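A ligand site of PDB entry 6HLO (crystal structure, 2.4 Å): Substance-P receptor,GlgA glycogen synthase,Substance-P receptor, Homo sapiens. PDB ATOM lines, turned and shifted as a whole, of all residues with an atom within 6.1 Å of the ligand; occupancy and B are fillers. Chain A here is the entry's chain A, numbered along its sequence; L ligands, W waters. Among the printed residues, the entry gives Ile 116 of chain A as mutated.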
ATOM      1  N   MET A  81      -4.006  26.316 -27.591  1.00  0.00           N
ATOM      2  CA  MET A  81      -5.158  25.921 -26.785  1.00  0.00           C
ATOM      3  C   MET A  81      -6.411  26.663 -27.239  1.00  0.00           C
ATOM      4  O   MET A  81      -7.468  26.046 -27.409  1.00  0.00           O
ATOM      5  CB  MET A  81      -4.904  26.170 -25.298  1.00  0.00           C
ATOM      6  CG  MET A  81      -5.921  25.448 -24.414  1.00  0.00           C
ATOM      7  SD  MET A  81      -5.773  25.786 -22.649  1.00  0.00           S
ATOM      8  CE  MET A  81      -6.721  27.303 -22.522  1.00  0.00           C
ATOM      9  N   ASN A  85      -9.261  24.082 -28.701  1.00  0.00           N
ATOM     10  CA  ASN A  85     -10.111  23.527 -27.654  1.00  0.00           C
ATOM     11  C   ASN A  85     -11.371  24.349 -27.395  1.00  0.00           C
ATOM     12  O   ASN A  85     -12.375  23.799 -26.946  1.00  0.00           O
ATOM     13  CB  ASN A  85      -9.316  23.383 -26.364  1.00  0.00           C
ATOM     14  CG  ASN A  85      -8.201  22.357 -26.476  1.00  0.00           C
ATOM     15  OD1 ASN A  85      -7.050  22.716 -26.720  1.00  0.00           O
ATOM     16  ND2 ASN A  85      -8.538  21.080 -26.313  1.00  0.00           N
ATOM     17  N   ASN A  89     -15.144  22.971 -26.468  1.00  0.00           N
ATOM     18  CA  ASN A  89     -15.460  23.155 -25.060  1.00  0.00           C
ATOM     19  C   ASN A  89     -16.783  23.892 -24.895  1.00  0.00           C
ATOM     20  O   ASN A  89     -17.641  23.475 -24.116  1.00  0.00           O
ATOM     21  CB  ASN A  89     -14.324  23.904 -24.344  1.00  0.00           C
ATOM     22  CG  ASN A  89     -13.125  23.028 -24.085  1.00  0.00           C
ATOM     23  OD1 ASN A  89     -13.052  21.888 -24.539  1.00  0.00           O
ATOM     24  ND2 ASN A  89     -12.158  23.562 -23.337  1.00  0.00           N
ATOM     25  N   HIS A 108      -9.120  16.592 -26.213  1.00  0.00           N
ATOM     26  CA  HIS A 108      -9.871  17.587 -25.484  1.00  0.00           C
ATOM     27  C   HIS A 108      -9.631  17.483 -23.988  1.00  0.00           C
ATOM     28  O   HIS A 108      -9.623  18.503 -23.285  1.00  0.00           O
ATOM     29  CB  HIS A 108     -11.350  17.431 -25.868  1.00  0.00           C
ATOM     30  CG  HIS A 108     -12.336  17.750 -24.793  1.00  0.00           C
ATOM     31  ND1 HIS A 108     -12.962  18.977 -24.708  1.00  0.00           N
ATOM     32  CD2 HIS A 108     -12.854  16.998 -23.795  1.00  0.00           C
ATOM     33  CE1 HIS A 108     -13.805  18.966 -23.679  1.00  0.00           C
ATOM     34  NE2 HIS A 108     -13.756  17.773 -23.115  1.00  0.00           N
ATOM     35  N   ASN A 109      -9.406  16.276 -23.475  1.00  0.00           N
ATOM     36  CA  ASN A 109      -9.021  16.153 -22.074  1.00  0.00           C
ATOM     37  C   ASN A 109      -7.522  16.245 -21.816  1.00  0.00           C
ATOM     38  O   ASN A 109      -7.112  16.412 -20.666  1.00  0.00           O
ATOM     39  CB  ASN A 109      -9.562  14.846 -21.490  1.00  0.00           C
ATOM     40  CG  ASN A 109     -11.048  14.909 -21.238  1.00  0.00           C
ATOM     41  OD1 ASN A 109     -11.597  15.964 -20.951  1.00  0.00           O
ATOM     42  ND2 ASN A 109     -11.710  13.764 -21.363  1.00  0.00           N
ATOM     43  N   PHE A 110      -6.688  16.170 -22.859  1.00  0.00           N
ATOM     44  CA  PHE A 110      -5.248  16.091 -22.709  1.00  0.00           C
ATOM     45  C   PHE A 110      -4.548  17.431 -22.919  1.00  0.00           C
ATOM     46  O   PHE A 110      -3.790  17.878 -22.048  1.00  0.00           O
ATOM     47  CB  PHE A 110      -4.705  15.050 -23.698  1.00  0.00           C
ATOM     48  CG  PHE A 110      -3.202  15.023 -23.834  1.00  0.00           C
ATOM     49  CD1 PHE A 110      -2.555  15.825 -24.760  1.00  0.00           C
ATOM     50  CD2 PHE A 110      -2.438  14.158 -23.061  1.00  0.00           C
ATOM     51  CE1 PHE A 110      -1.181  15.793 -24.896  1.00  0.00           C
ATOM     52  CE2 PHE A 110      -1.065  14.112 -23.193  1.00  0.00           C
ATOM     53  CZ  PHE A 110      -0.433  14.934 -24.106  1.00  0.00           C
ATOM     54  N   PRO A 112      -5.180  20.815 -22.907  1.00  0.00           N
ATOM     55  CA  PRO A 112      -5.153  22.015 -22.060  1.00  0.00           C
ATOM     56  C   PRO A 112      -4.202  21.885 -20.875  1.00  0.00           C
ATOM     57  O   PRO A 112      -3.552  22.877 -20.510  1.00  0.00           O
ATOM     58  CB  PRO A 112      -6.611  22.137 -21.592  1.00  0.00           C
ATOM     59  CG  PRO A 112      -7.402  21.446 -22.629  1.00  0.00           C
ATOM     60  CD  PRO A 112      -6.553  20.300 -23.088  1.00  0.00           C
ATOM     61  N   ILE A 113      -4.076  20.700 -20.294  1.00  0.00           N
ATOM     62  CA  ILE A 113      -3.149  20.523 -19.170  1.00  0.00           C
ATOM     63  C   ILE A 113      -1.714  20.738 -19.635  1.00  0.00           C
ATOM     64  O   ILE A 113      -0.953  21.486 -19.010  1.00  0.00           O
ATOM     65  CB  ILE A 113      -3.350  19.140 -18.537  1.00  0.00           C
ATOM     66  CG1 ILE A 113      -4.665  19.102 -17.748  1.00  0.00           C
ATOM     67  CG2 ILE A 113      -2.183  18.775 -17.644  1.00  0.00           C
ATOM     68  CD1 ILE A 113      -5.046  17.735 -17.223  1.00  0.00           C
ATOM     69  N   ILE A 116      -1.220  24.636 -20.597  1.00  0.00           N
ATOM     70  CA  ILE A 116      -1.118  25.521 -19.439  1.00  0.00           C
ATOM     71  C   ILE A 116       0.166  25.242 -18.668  1.00  0.00           C
ATOM     72  O   ILE A 116       0.813  26.173 -18.168  1.00  0.00           O
ATOM     73  CB  ILE A 116      -2.370  25.381 -18.557  1.00  0.00           C
ATOM     74  CG1 ILE A 116      -3.612  25.812 -19.331  1.00  0.00           C
ATOM     75  CG2 ILE A 116      -2.215  26.183 -17.272  1.00  0.00           C
ATOM     76  CD1 ILE A 116      -3.460  27.139 -20.057  1.00  0.00           C
ATOM     77  N   PHE A 117       0.580  23.971 -18.591  1.00  0.00           N
ATOM     78  CA  PHE A 117       1.840  23.650 -17.936  1.00  0.00           C
ATOM     79  C   PHE A 117       3.000  24.332 -18.655  1.00  0.00           C
ATOM     80  O   PHE A 117       3.830  25.000 -18.029  1.00  0.00           O
ATOM     81  CB  PHE A 117       2.044  22.134 -17.905  1.00  0.00           C
ATOM     82  CG  PHE A 117       3.268  21.688 -17.160  1.00  0.00           C
ATOM     83  CD1 PHE A 117       4.519  21.716 -17.761  1.00  0.00           C
ATOM     84  CD2 PHE A 117       3.175  21.216 -15.862  1.00  0.00           C
ATOM     85  CE1 PHE A 117       5.644  21.292 -17.086  1.00  0.00           C
ATOM     86  CE2 PHE A 117       4.299  20.798 -15.168  1.00  0.00           C
ATOM     87  CZ  PHE A 117       5.538  20.838 -15.785  1.00  0.00           C
ATOM     88  N   PRO A 164      -2.037  10.832 -18.316  1.00  0.00           N
ATOM     89  CA  PRO A 164      -3.063   9.971 -17.705  1.00  0.00           C
ATOM     90  C   PRO A 164      -4.490  10.427 -17.977  1.00  0.00           C
ATOM     91  O   PRO A 164      -5.389   9.587 -18.110  1.00  0.00           O
ATOM     92  CB  PRO A 164      -2.732  10.040 -16.204  1.00  0.00           C
ATOM     93  CG  PRO A 164      -1.300  10.431 -16.145  1.00  0.00           C
ATOM     94  CD  PRO A 164      -1.099  11.362 -17.306  1.00  0.00           C
ATOM     95  N   GLN A 165      -4.718  11.732 -18.047  1.00  0.00           N
ATOM     96  CA  GLN A 165      -6.069  12.231 -18.283  1.00  0.00           C
ATOM     97  C   GLN A 165      -6.538  11.951 -19.708  1.00  0.00           C
ATOM     98  O   GLN A 165      -7.725  11.674 -19.938  1.00  0.00           O
ATOM     99  CB  GLN A 165      -6.125  13.736 -17.989  1.00  0.00           C
ATOM    100  CG  GLN A 165      -7.487  14.357 -18.150  1.00  0.00           C
ATOM    101  CD  GLN A 165      -7.722  15.474 -17.155  1.00  0.00           C
ATOM    102  OE1 GLN A 165      -7.176  15.471 -16.063  1.00  0.00           O
ATOM    103  NE2 GLN A 165      -8.539  16.450 -17.546  1.00  0.00           N
ATOM    104  N   ILE A 182     -13.729  10.710 -18.484  1.00  0.00           N
ATOM    105  CA  ILE A 182     -12.481  10.153 -17.986  1.00  0.00           C
ATOM    106  C   ILE A 182     -12.811   8.957 -17.099  1.00  0.00           C
ATOM    107  O   ILE A 182     -13.498   9.104 -16.075  1.00  0.00           O
ATOM    108  CB  ILE A 182     -11.669  11.198 -17.210  1.00  0.00           C
ATOM    109  CG1 ILE A 182     -11.550  12.482 -18.031  1.00  0.00           C
ATOM    110  CG2 ILE A 182     -10.281  10.661 -16.873  1.00  0.00           C
ATOM    111  CD1 ILE A 182     -10.895  13.626 -17.282  1.00  0.00           C
ATOM    112  N   TRP A 184     -11.095   6.254 -15.015  1.00  0.00           N
ATOM    113  CA  TRP A 184      -9.995   5.616 -14.315  1.00  0.00           C
ATOM    114  C   TRP A 184     -10.360   4.183 -13.946  1.00  0.00           C
ATOM    115  O   TRP A 184     -11.543   3.858 -13.790  1.00  0.00           O
ATOM    116  CB  TRP A 184      -9.637   6.409 -13.059  1.00  0.00           C
ATOM    117  CG  TRP A 184      -8.901   7.671 -13.366  1.00  0.00           C
ATOM    118  CD1 TRP A 184      -9.415   8.799 -13.935  1.00  0.00           C
ATOM    119  CD2 TRP A 184      -7.522   7.928 -13.131  1.00  0.00           C
ATOM    120  NE1 TRP A 184      -8.431   9.747 -14.072  1.00  0.00           N
ATOM    121  CE2 TRP A 184      -7.253   9.240 -13.575  1.00  0.00           C
ATOM    122  CE3 TRP A 184      -6.473   7.180 -12.579  1.00  0.00           C
ATOM    123  CZ2 TRP A 184      -5.994   9.819 -13.501  1.00  0.00           C
ATOM    124  CZ3 TRP A 184      -5.215   7.762 -12.495  1.00  0.00           C
ATOM    125  CH2 TRP A 184      -4.994   9.066 -12.952  1.00  0.00           C
ATOM    126  N   GLU A 193      -7.351   8.780  -9.080  1.00  0.00           N
ATOM    127  CA  GLU A 193      -7.831   9.897  -9.885  1.00  0.00           C
ATOM    128  C   GLU A 193      -7.838  11.189  -9.083  1.00  0.00           C
ATOM    129  O   GLU A 193      -7.477  12.256  -9.596  1.00  0.00           O
ATOM    130  CB  GLU A 193      -9.229   9.569 -10.416  1.00  0.00           C
ATOM    131  CG  GLU A 193      -9.954  10.730 -11.049  1.00  0.00           C
ATOM    132  CD  GLU A 193     -11.285  10.327 -11.633  1.00  0.00           C
ATOM    133  OE1 GLU A 193     -11.875  11.153 -12.375  1.00  0.00           O
ATOM    134  OE2 GLU A 193     -11.741   9.194 -11.371  1.00  0.00           O
ATOM    135  N   TYR A 196      -4.294  12.414  -8.608  1.00  0.00           N
ATOM    136  CA  TYR A 196      -3.804  12.941  -9.873  1.00  0.00           C
ATOM    137  C   TYR A 196      -4.349  14.342 -10.132  1.00  0.00           C
ATOM    138  O   TYR A 196      -3.607  15.233 -10.550  1.00  0.00           O
ATOM    139  CB  TYR A 196      -4.192  12.006 -11.022  1.00  0.00           C
ATOM    140  CG  TYR A 196      -3.945  12.594 -12.384  1.00  0.00           C
ATOM    141  CD1 TYR A 196      -4.987  13.121 -13.138  1.00  0.00           C
ATOM    142  CD2 TYR A 196      -2.672  12.624 -12.931  1.00  0.00           C
ATOM    143  CE1 TYR A 196      -4.762  13.667 -14.382  1.00  0.00           C
ATOM    144  CE2 TYR A 196      -2.433  13.169 -14.174  1.00  0.00           C
ATOM    145  CZ  TYR A 196      -3.485  13.682 -14.903  1.00  0.00           C
ATOM    146  OH  TYR A 196      -3.246  14.227 -16.146  1.00  0.00           O
ATOM    147  N   HIS A 197      -5.638  14.548  -9.876  1.00  0.00           N
ATOM    148  CA  HIS A 197      -6.221  15.865 -10.080  1.00  0.00           C
ATOM    149  C   HIS A 197      -5.612  16.899  -9.152  1.00  0.00           C
ATOM    150  O   HIS A 197      -5.288  18.014  -9.569  1.00  0.00           O
ATOM    151  CB  HIS A 197      -7.740  15.797  -9.894  1.00  0.00           C
ATOM    152  CG  HIS A 197      -8.414  17.134  -9.988  1.00  0.00           C
ATOM    153  ND1 HIS A 197      -9.546  17.441  -9.262  1.00  0.00           N
ATOM    154  CD2 HIS A 197      -8.126  18.239 -10.722  1.00  0.00           C
ATOM    155  CE1 HIS A 197      -9.925  18.676  -9.535  1.00  0.00           C
ATOM    156  NE2 HIS A 197      -9.080  19.180 -10.419  1.00  0.00           N
ATOM    157  N   VAL A 200      -2.104  17.771 -10.415  1.00  0.00           N
ATOM    158  CA  VAL A 200      -2.095  18.642 -11.598  1.00  0.00           C
ATOM    159  C   VAL A 200      -2.449  20.064 -11.212  1.00  0.00           C
ATOM    160  O   VAL A 200      -1.813  21.024 -11.673  1.00  0.00           O
ATOM    161  CB  VAL A 200      -3.054  18.091 -12.678  1.00  0.00           C
ATOM    162  CG1 VAL A 200      -3.158  19.086 -13.828  1.00  0.00           C
ATOM    163  CG2 VAL A 200      -2.570  16.742 -13.180  1.00  0.00           C
ATOM    164  N   THR A 201      -3.440  20.226 -10.329  1.00  0.00           N
ATOM    165  CA  THR A 201      -3.808  21.578  -9.910  1.00  0.00           C
ATOM    166  C   THR A 201      -2.670  22.266  -9.175  1.00  0.00           C
ATOM    167  O   THR A 201      -2.480  23.485  -9.322  1.00  0.00           O
ATOM    168  CB  THR A 201      -5.064  21.521  -9.025  1.00  0.00           C
ATOM    169  OG1 THR A 201      -6.147  20.952  -9.772  1.00  0.00           O
ATOM    170  CG2 THR A 201      -5.468  22.920  -8.583  1.00  0.00           C
ATOM    171  N   VAL A 202      -1.887  21.516  -8.406  1.00  0.00           N
ATOM    172  CA  VAL A 202      -0.745  22.126  -7.729  1.00  0.00           C
ATOM    173  C   VAL A 202       0.344  22.492  -8.733  1.00  0.00           C
ATOM    174  O   VAL A 202       0.901  23.600  -8.701  1.00  0.00           O
ATOM    175  CB  VAL A 202      -0.206  21.189  -6.628  1.00  0.00           C
ATOM    176  CG1 VAL A 202       1.128  21.683  -6.106  1.00  0.00           C
ATOM    177  CG2 VAL A 202      -1.208  21.076  -5.488  1.00  0.00           C
ATOM    178  N   ILE A 204       0.285  23.084 -11.988  1.00  0.00           N
ATOM    179  CA  ILE A 204       0.009  24.107 -12.995  1.00  0.00           C
ATOM    180  C   ILE A 204      -0.608  25.365 -12.413  1.00  0.00           C
ATOM    181  O   ILE A 204      -0.902  26.308 -13.163  1.00  0.00           O
ATOM    182  CB  ILE A 204      -0.887  23.549 -14.129  1.00  0.00           C
ATOM    183  CG1 ILE A 204      -2.328  23.390 -13.652  1.00  0.00           C
ATOM    184  CG2 ILE A 204      -0.327  22.244 -14.660  1.00  0.00           C
ATOM    185  CD1 ILE A 204      -3.286  22.987 -14.758  1.00  0.00           C
ATOM    186  N   TRP A 446      -7.424  31.961 -13.590  1.00  0.00           N
ATOM    187  CA  TRP A 446      -7.550  30.540 -13.317  1.00  0.00           C
ATOM    188  C   TRP A 446      -8.062  30.190 -11.923  1.00  0.00           C
ATOM    189  O   TRP A 446      -8.463  29.043 -11.714  1.00  0.00           O
ATOM    190  CB  TRP A 446      -6.215  29.832 -13.574  1.00  0.00           C
ATOM    191  CG  TRP A 446      -5.941  29.701 -15.037  1.00  0.00           C
ATOM    192  CD1 TRP A 446      -5.103  30.475 -15.776  1.00  0.00           C
ATOM    193  CD2 TRP A 446      -6.536  28.762 -15.942  1.00  0.00           C
ATOM    194  NE1 TRP A 446      -5.125  30.069 -17.094  1.00  0.00           N
ATOM    195  CE2 TRP A 446      -5.990  29.021 -17.218  1.00  0.00           C
ATOM    196  CE3 TRP A 446      -7.458  27.728 -15.802  1.00  0.00           C
ATOM    197  CZ2 TRP A 446      -6.353  28.278 -18.344  1.00  0.00           C
ATOM    198  CZ3 TRP A 446      -7.822  26.989 -16.918  1.00  0.00           C
ATOM    199  CH2 TRP A 446      -7.264  27.266 -18.178  1.00  0.00           C
ATOM    200  N   PHE A 449     -11.689  28.651 -11.838  1.00  0.00           N
ATOM    201  CA  PHE A 449     -11.754  27.348 -12.507  1.00  0.00           C
ATOM    202  C   PHE A 449     -11.310  26.222 -11.575  1.00  0.00           C
ATOM    203  O   PHE A 449     -12.015  25.220 -11.403  1.00  0.00           O
ATOM    204  CB  PHE A 449     -10.876  27.425 -13.764  1.00  0.00           C
ATOM    205  CG  PHE A 449     -10.895  26.199 -14.623  1.00  0.00           C
ATOM    206  CD1 PHE A 449      -9.948  25.197 -14.442  1.00  0.00           C
ATOM    207  CD2 PHE A 449     -11.816  26.062 -15.654  1.00  0.00           C
ATOM    208  CE1 PHE A 449      -9.941  24.073 -15.257  1.00  0.00           C
ATOM    209  CE2 PHE A 449     -11.815  24.945 -16.472  1.00  0.00           C
ATOM    210  CZ  PHE A 449     -10.870  23.950 -16.273  1.00  0.00           C
ATOM    211  N   HIS A 450     -10.149  26.395 -10.954  1.00  0.00           N
ATOM    212  CA  HIS A 450      -9.666  25.398 -10.008  1.00  0.00           C
ATOM    213  C   HIS A 450     -10.535  25.321  -8.771  1.00  0.00           C
ATOM    214  O   HIS A 450     -10.710  24.233  -8.210  1.00  0.00           O
ATOM    215  CB  HIS A 450      -8.215  25.689  -9.650  1.00  0.00           C
ATOM    216  CG  HIS A 450      -7.260  25.502 -10.783  1.00  0.00           C
ATOM    217  ND1 HIS A 450      -7.027  24.273 -11.361  1.00  0.00           N
ATOM    218  CD2 HIS A 450      -6.496  26.390 -11.461  1.00  0.00           C
ATOM    219  CE1 HIS A 450      -6.149  24.409 -12.342  1.00  0.00           C
ATOM    220  NE2 HIS A 450      -5.807  25.681 -12.428  1.00  0.00           N
ATOM    221  N   PHE A 453     -13.470  23.132  -9.724  1.00  0.00           N
ATOM    222  CA  PHE A 453     -13.204  21.696  -9.777  1.00  0.00           C
ATOM    223  C   PHE A 453     -12.727  21.109  -8.458  1.00  0.00           C
ATOM    224  O   PHE A 453     -12.746  19.877  -8.311  1.00  0.00           O
ATOM    225  CB  PHE A 453     -12.214  21.378 -10.894  1.00  0.00           C
ATOM    226  CG  PHE A 453     -12.861  21.289 -12.252  1.00  0.00           C
ATOM    227  CD1 PHE A 453     -13.575  20.155 -12.608  1.00  0.00           C
ATOM    228  CD2 PHE A 453     -12.800  22.347 -13.142  1.00  0.00           C
ATOM    229  CE1 PHE A 453     -14.192  20.071 -13.848  1.00  0.00           C
ATOM    230  CE2 PHE A 453     -13.403  22.262 -14.380  1.00  0.00           C
ATOM    231  CZ  PHE A 453     -14.111  21.122 -14.733  1.00  0.00           C
ATOM    232  N   TYR A 457     -14.608  18.147  -3.493  1.00  0.00           N
ATOM    233  CA  TYR A 457     -13.831  17.441  -2.475  1.00  0.00           C
ATOM    234  C   TYR A 457     -14.151  17.925  -1.059  1.00  0.00           C
ATOM    235  O   TYR A 457     -13.995  17.155  -0.104  1.00  0.00           O
ATOM    236  CB  TYR A 457     -12.334  17.592  -2.754  1.00  0.00           C
ATOM    237  CG  TYR A 457     -11.893  17.004  -4.071  1.00  0.00           C
ATOM    238  CD1 TYR A 457     -12.572  15.936  -4.656  1.00  0.00           C
ATOM    239  CD2 TYR A 457     -10.788  17.513  -4.739  1.00  0.00           C
ATOM    240  CE1 TYR A 457     -12.170  15.400  -5.867  1.00  0.00           C
ATOM    241  CE2 TYR A 457     -10.371  16.990  -5.952  1.00  0.00           C
ATOM    242  CZ  TYR A 457     -11.072  15.939  -6.514  1.00  0.00           C
ATOM    243  OH  TYR A 457     -10.664  15.412  -7.717  1.00  0.00           O
ATOM    244  N   TYR A 472     -20.813  27.712 -15.020  1.00  0.00           N
ATOM    245  CA  TYR A 472     -19.689  27.042 -15.671  1.00  0.00           C
ATOM    246  C   TYR A 472     -19.270  27.758 -16.941  1.00  0.00           C
ATOM    247  O   TYR A 472     -18.072  27.850 -17.241  1.00  0.00           O
ATOM    248  CB  TYR A 472     -20.042  25.591 -15.982  1.00  0.00           C
ATOM    249  CG  TYR A 472     -18.885  24.832 -16.578  1.00  0.00           C
ATOM    250  CD1 TYR A 472     -18.859  24.503 -17.927  1.00  0.00           C
ATOM    251  CD2 TYR A 472     -17.790  24.482 -15.793  1.00  0.00           C
ATOM    252  CE1 TYR A 472     -17.783  23.818 -18.471  1.00  0.00           C
ATOM    253  CE2 TYR A 472     -16.715  23.801 -16.328  1.00  0.00           C
ATOM    254  CZ  TYR A 472     -16.718  23.476 -17.670  1.00  0.00           C
ATOM    255  OH  TYR A 472     -15.652  22.794 -18.185  1.00  0.00           O
ATOM    256  N   MET A 476     -15.557  29.043 -17.240  1.00  0.00           N
ATOM    257  CA  MET A 476     -14.752  28.554 -18.352  1.00  0.00           C
ATOM    258  C   MET A 476     -14.334  29.685 -19.283  1.00  0.00           C
ATOM    259  O   MET A 476     -13.209  29.695 -19.785  1.00  0.00           O
ATOM    260  CB  MET A 476     -15.523  27.478 -19.124  1.00  0.00           C
ATOM    261  CG  MET A 476     -14.931  27.167 -20.495  1.00  0.00           C
ATOM    262  SD  MET A 476     -15.452  25.565 -21.133  1.00  0.00           S
ATOM    263  CE  MET A 476     -14.250  24.504 -20.337  1.00  0.00           C
ATOM    264  N   ALA A 479     -11.361  31.523 -17.650  1.00  0.00           N
ATOM    265  CA  ALA A 479     -10.119  30.755 -17.674  1.00  0.00           C
ATOM    266  C   ALA A 479      -9.498  30.763 -19.063  1.00  0.00           C
ATOM    267  O   ALA A 479      -8.297  31.021 -19.216  1.00  0.00           O
ATOM    268  CB  ALA A 479     -10.388  29.322 -17.211  1.00  0.00           C
ATOM    269  N   MET A 480     -10.304  30.493 -20.092  1.00  0.00           N
ATOM    270  CA  MET A 480      -9.780  30.481 -21.451  1.00  0.00           C
ATOM    271  C   MET A 480      -9.477  31.877 -21.973  1.00  0.00           C
ATOM    272  O   MET A 480      -8.663  32.023 -22.890  1.00  0.00           O
ATOM    273  CB  MET A 480     -10.769  29.764 -22.384  1.00  0.00           C
ATOM    274  CG  MET A 480     -11.147  28.371 -21.892  1.00  0.00           C
ATOM    275  SD  MET A 480     -11.664  27.269 -23.222  1.00  0.00           S
ATOM    276  CE  MET A 480     -10.124  27.086 -24.116  1.00  0.00           C
HETATM  277  C1  LIG L   1      -6.446  22.941 -16.997  1.00  0.00           C
HETATM  278  C2  LIG L   1     -11.701  16.695 -15.387  1.00  0.00           C
HETATM  279  C3  LIG L   1     -12.032  17.160 -16.778  1.00  0.00           C
HETATM  280  C4  LIG L   1     -10.341  16.872 -13.500  1.00  0.00           C
HETATM  281  C5  LIG L   1      -9.408  18.756 -19.562  1.00  0.00           C
HETATM  282  C6  LIG L   1     -10.126  19.706 -18.572  1.00  0.00           C
HETATM  283  C7  LIG L   1      -9.450  21.126 -18.609  1.00  0.00           C
HETATM  284  C8  LIG L   1      -8.308  21.416 -17.838  1.00  0.00           C
HETATM  285  C9  LIG L   1      -7.702  22.684 -17.875  1.00  0.00           C
HETATM  286  C10 LIG L   1      -8.205  23.699 -18.702  1.00  0.00           C
HETATM  287  C11 LIG L   1      -9.344  23.420 -19.486  1.00  0.00           C
HETATM  288  C12 LIG L   1      -9.959  22.148 -19.439  1.00  0.00           C
HETATM  289  C13 LIG L   1      -9.926  24.524 -20.403  1.00  0.00           C
HETATM  290  C14 LIG L   1     -11.097  19.338 -16.340  1.00  0.00           C
HETATM  291  C15 LIG L   1     -10.639  18.900 -14.860  1.00  0.00           C
HETATM  292  C16 LIG L   1     -10.177  15.352 -13.493  1.00  0.00           C
HETATM  293  C17 LIG L   1      -9.278  13.302 -13.926  1.00  0.00           C
HETATM  294  C18 LIG L   1      -9.286  19.490 -14.357  1.00  0.00           C
HETATM  295  C19 LIG L   1      -9.220  20.615 -13.503  1.00  0.00           C
HETATM  296  C20 LIG L   1      -7.998  21.164 -13.041  1.00  0.00           C
HETATM  297  C21 LIG L   1      -6.805  20.572 -13.456  1.00  0.00           C
HETATM  298  C22 LIG L   1      -6.793  19.449 -14.313  1.00  0.00           C
HETATM  299  C23 LIG L   1      -8.029  18.936 -14.757  1.00  0.00           C
HETATM  300  F1  LIG L   1      -9.817  24.331 -21.746  1.00  0.00           F
HETATM  301  F2  LIG L   1      -9.377  25.759 -20.256  1.00  0.00           F
HETATM  302  F3  LIG L   1     -11.242  24.797 -20.267  1.00  0.00           F
HETATM  303  F4  LIG L   1      -6.638  23.679 -15.873  1.00  0.00           F
HETATM  304  F5  LIG L   1      -5.823  21.841 -16.500  1.00  0.00           F
HETATM  305  F6  LIG L   1      -5.401  23.583 -17.588  1.00  0.00           F
HETATM  306  F7  LIG L   1      -5.617  21.091 -13.030  1.00  0.00           F
HETATM  307  N1  LIG L   1     -10.488  17.393 -14.859  1.00  0.00           N
HETATM  308  N2  LIG L   1      -9.114  14.699 -14.103  1.00  0.00           N
HETATM  309  N3  LIG L   1     -10.494  13.108 -13.182  1.00  0.00           N
HETATM  310  N4  LIG L   1     -11.038  14.397 -12.930  1.00  0.00           N
HETATM  311  O1  LIG L   1     -10.046  19.112 -17.270  1.00  0.00           O
HETATM  312  O2  LIG L   1     -12.202  18.567 -16.770  1.00  0.00           O
HETATM  313  O3  LIG L   1      -8.565  12.378 -14.302  1.00  0.00           O
HETATM  314  O   HOH W   1      -8.627  22.050 -10.023  1.00  0.00           O
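The side-chain amide oxygen of Gln 165 lies close to a nitrogen (N2) of the ligand. An oxygen (O3) of the ligand sits at hydrogen-bond distance from the indole nitrogen (NE1) of Trp 184 (2.6 Å). The side-chain carboxylate of Glu 193 is in hydrogen-bond range of a nitrogen (N3) of the ligand (2.5 Å).
A ring nitrogen (ND1) of His 108 is in hydrogen-bond range of the side-chain amide oxygen (OD1) of Asn 89. The backbone carbonyl oxygen of Met 81 lies close to the side-chain amide oxygen of Asn 85, at 3.4 Å. The backbone carbonyl oxygen (O) of His 197 lies within hydrogen-bond range of the side-chain hydroxyl (OG1) of Thr 201, 3.1 Å away. The side-chain amide oxygen (OD1) of Asn 89 lies close to the backbone carbonyl oxygen (O) of Asn 85, 3.1 Å away. O of Asn 109 sits close to NE2 of Gln 165 (3.4 Å). The side-chain sulfur (SD) of Met 480 sits at hydrogen-bond distance from the side-chain amide nitrogen (ND2) of Asn 89, at 3.7 Å. The backbone NH (N) of Gln 165 sits close to the side-chain hydroxyl (OH) of Tyr 196, 3.5 Å away. A ring nitrogen (ND1) of His 197 sits at hydrogen-bond distance from the side-chain hydroxyl of Tyr 457 (2.8 Å).
A fluorine (F1) of the ligand sits close to the side-chain amide nitrogen of Asn 89. The side-chain hydroxyl of Thr 201 sits close to a fluorine (F7) of the ligand (3.3 Å). The side-chain sulfur (SD) of Met 480 lies close to a fluorine (F1) of the ligand, 3.8 Å away. Merely in contact with the ligand: Met 476 (3.0 Å), Ile 113 (3.2 Å), Val 200 (3.3 Å), Ile 204 (3.3 Å), Trp 446 (3.3 Å), Ile 116 (3.3 Å), Phe 449 (3.4 Å), His 197 (3.4 Å), His 450 (3.4 Å), Asn 109 (3.5 Å), Pro 112 (3.5 Å), Ile 182 (3.5 Å), His 108 (3.7 Å), Phe 453 (3.8 Å), Met 81 (3.8 Å) and Tyr 196 (3.8 Å). Hydrophobic or aromatic side chains that line the ligand: Met 81, Pro 112, Ile 113, Ile 116, Ile 182, Trp 184, Tyr 196, His 197, Val 200, Ile 204, Trp 446, Phe 449, His 450, Phe 453, Met 476 and Met 480. Of the 30 residues printed, 22 come within 4 Å of the ligand.
Water W1 lies within hydrogen-bond range of OG1 of Thr 201 (2.7 Å), NE2 of His 197 (2.9 Å) and ND1 of His 450 (3.0 Å).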
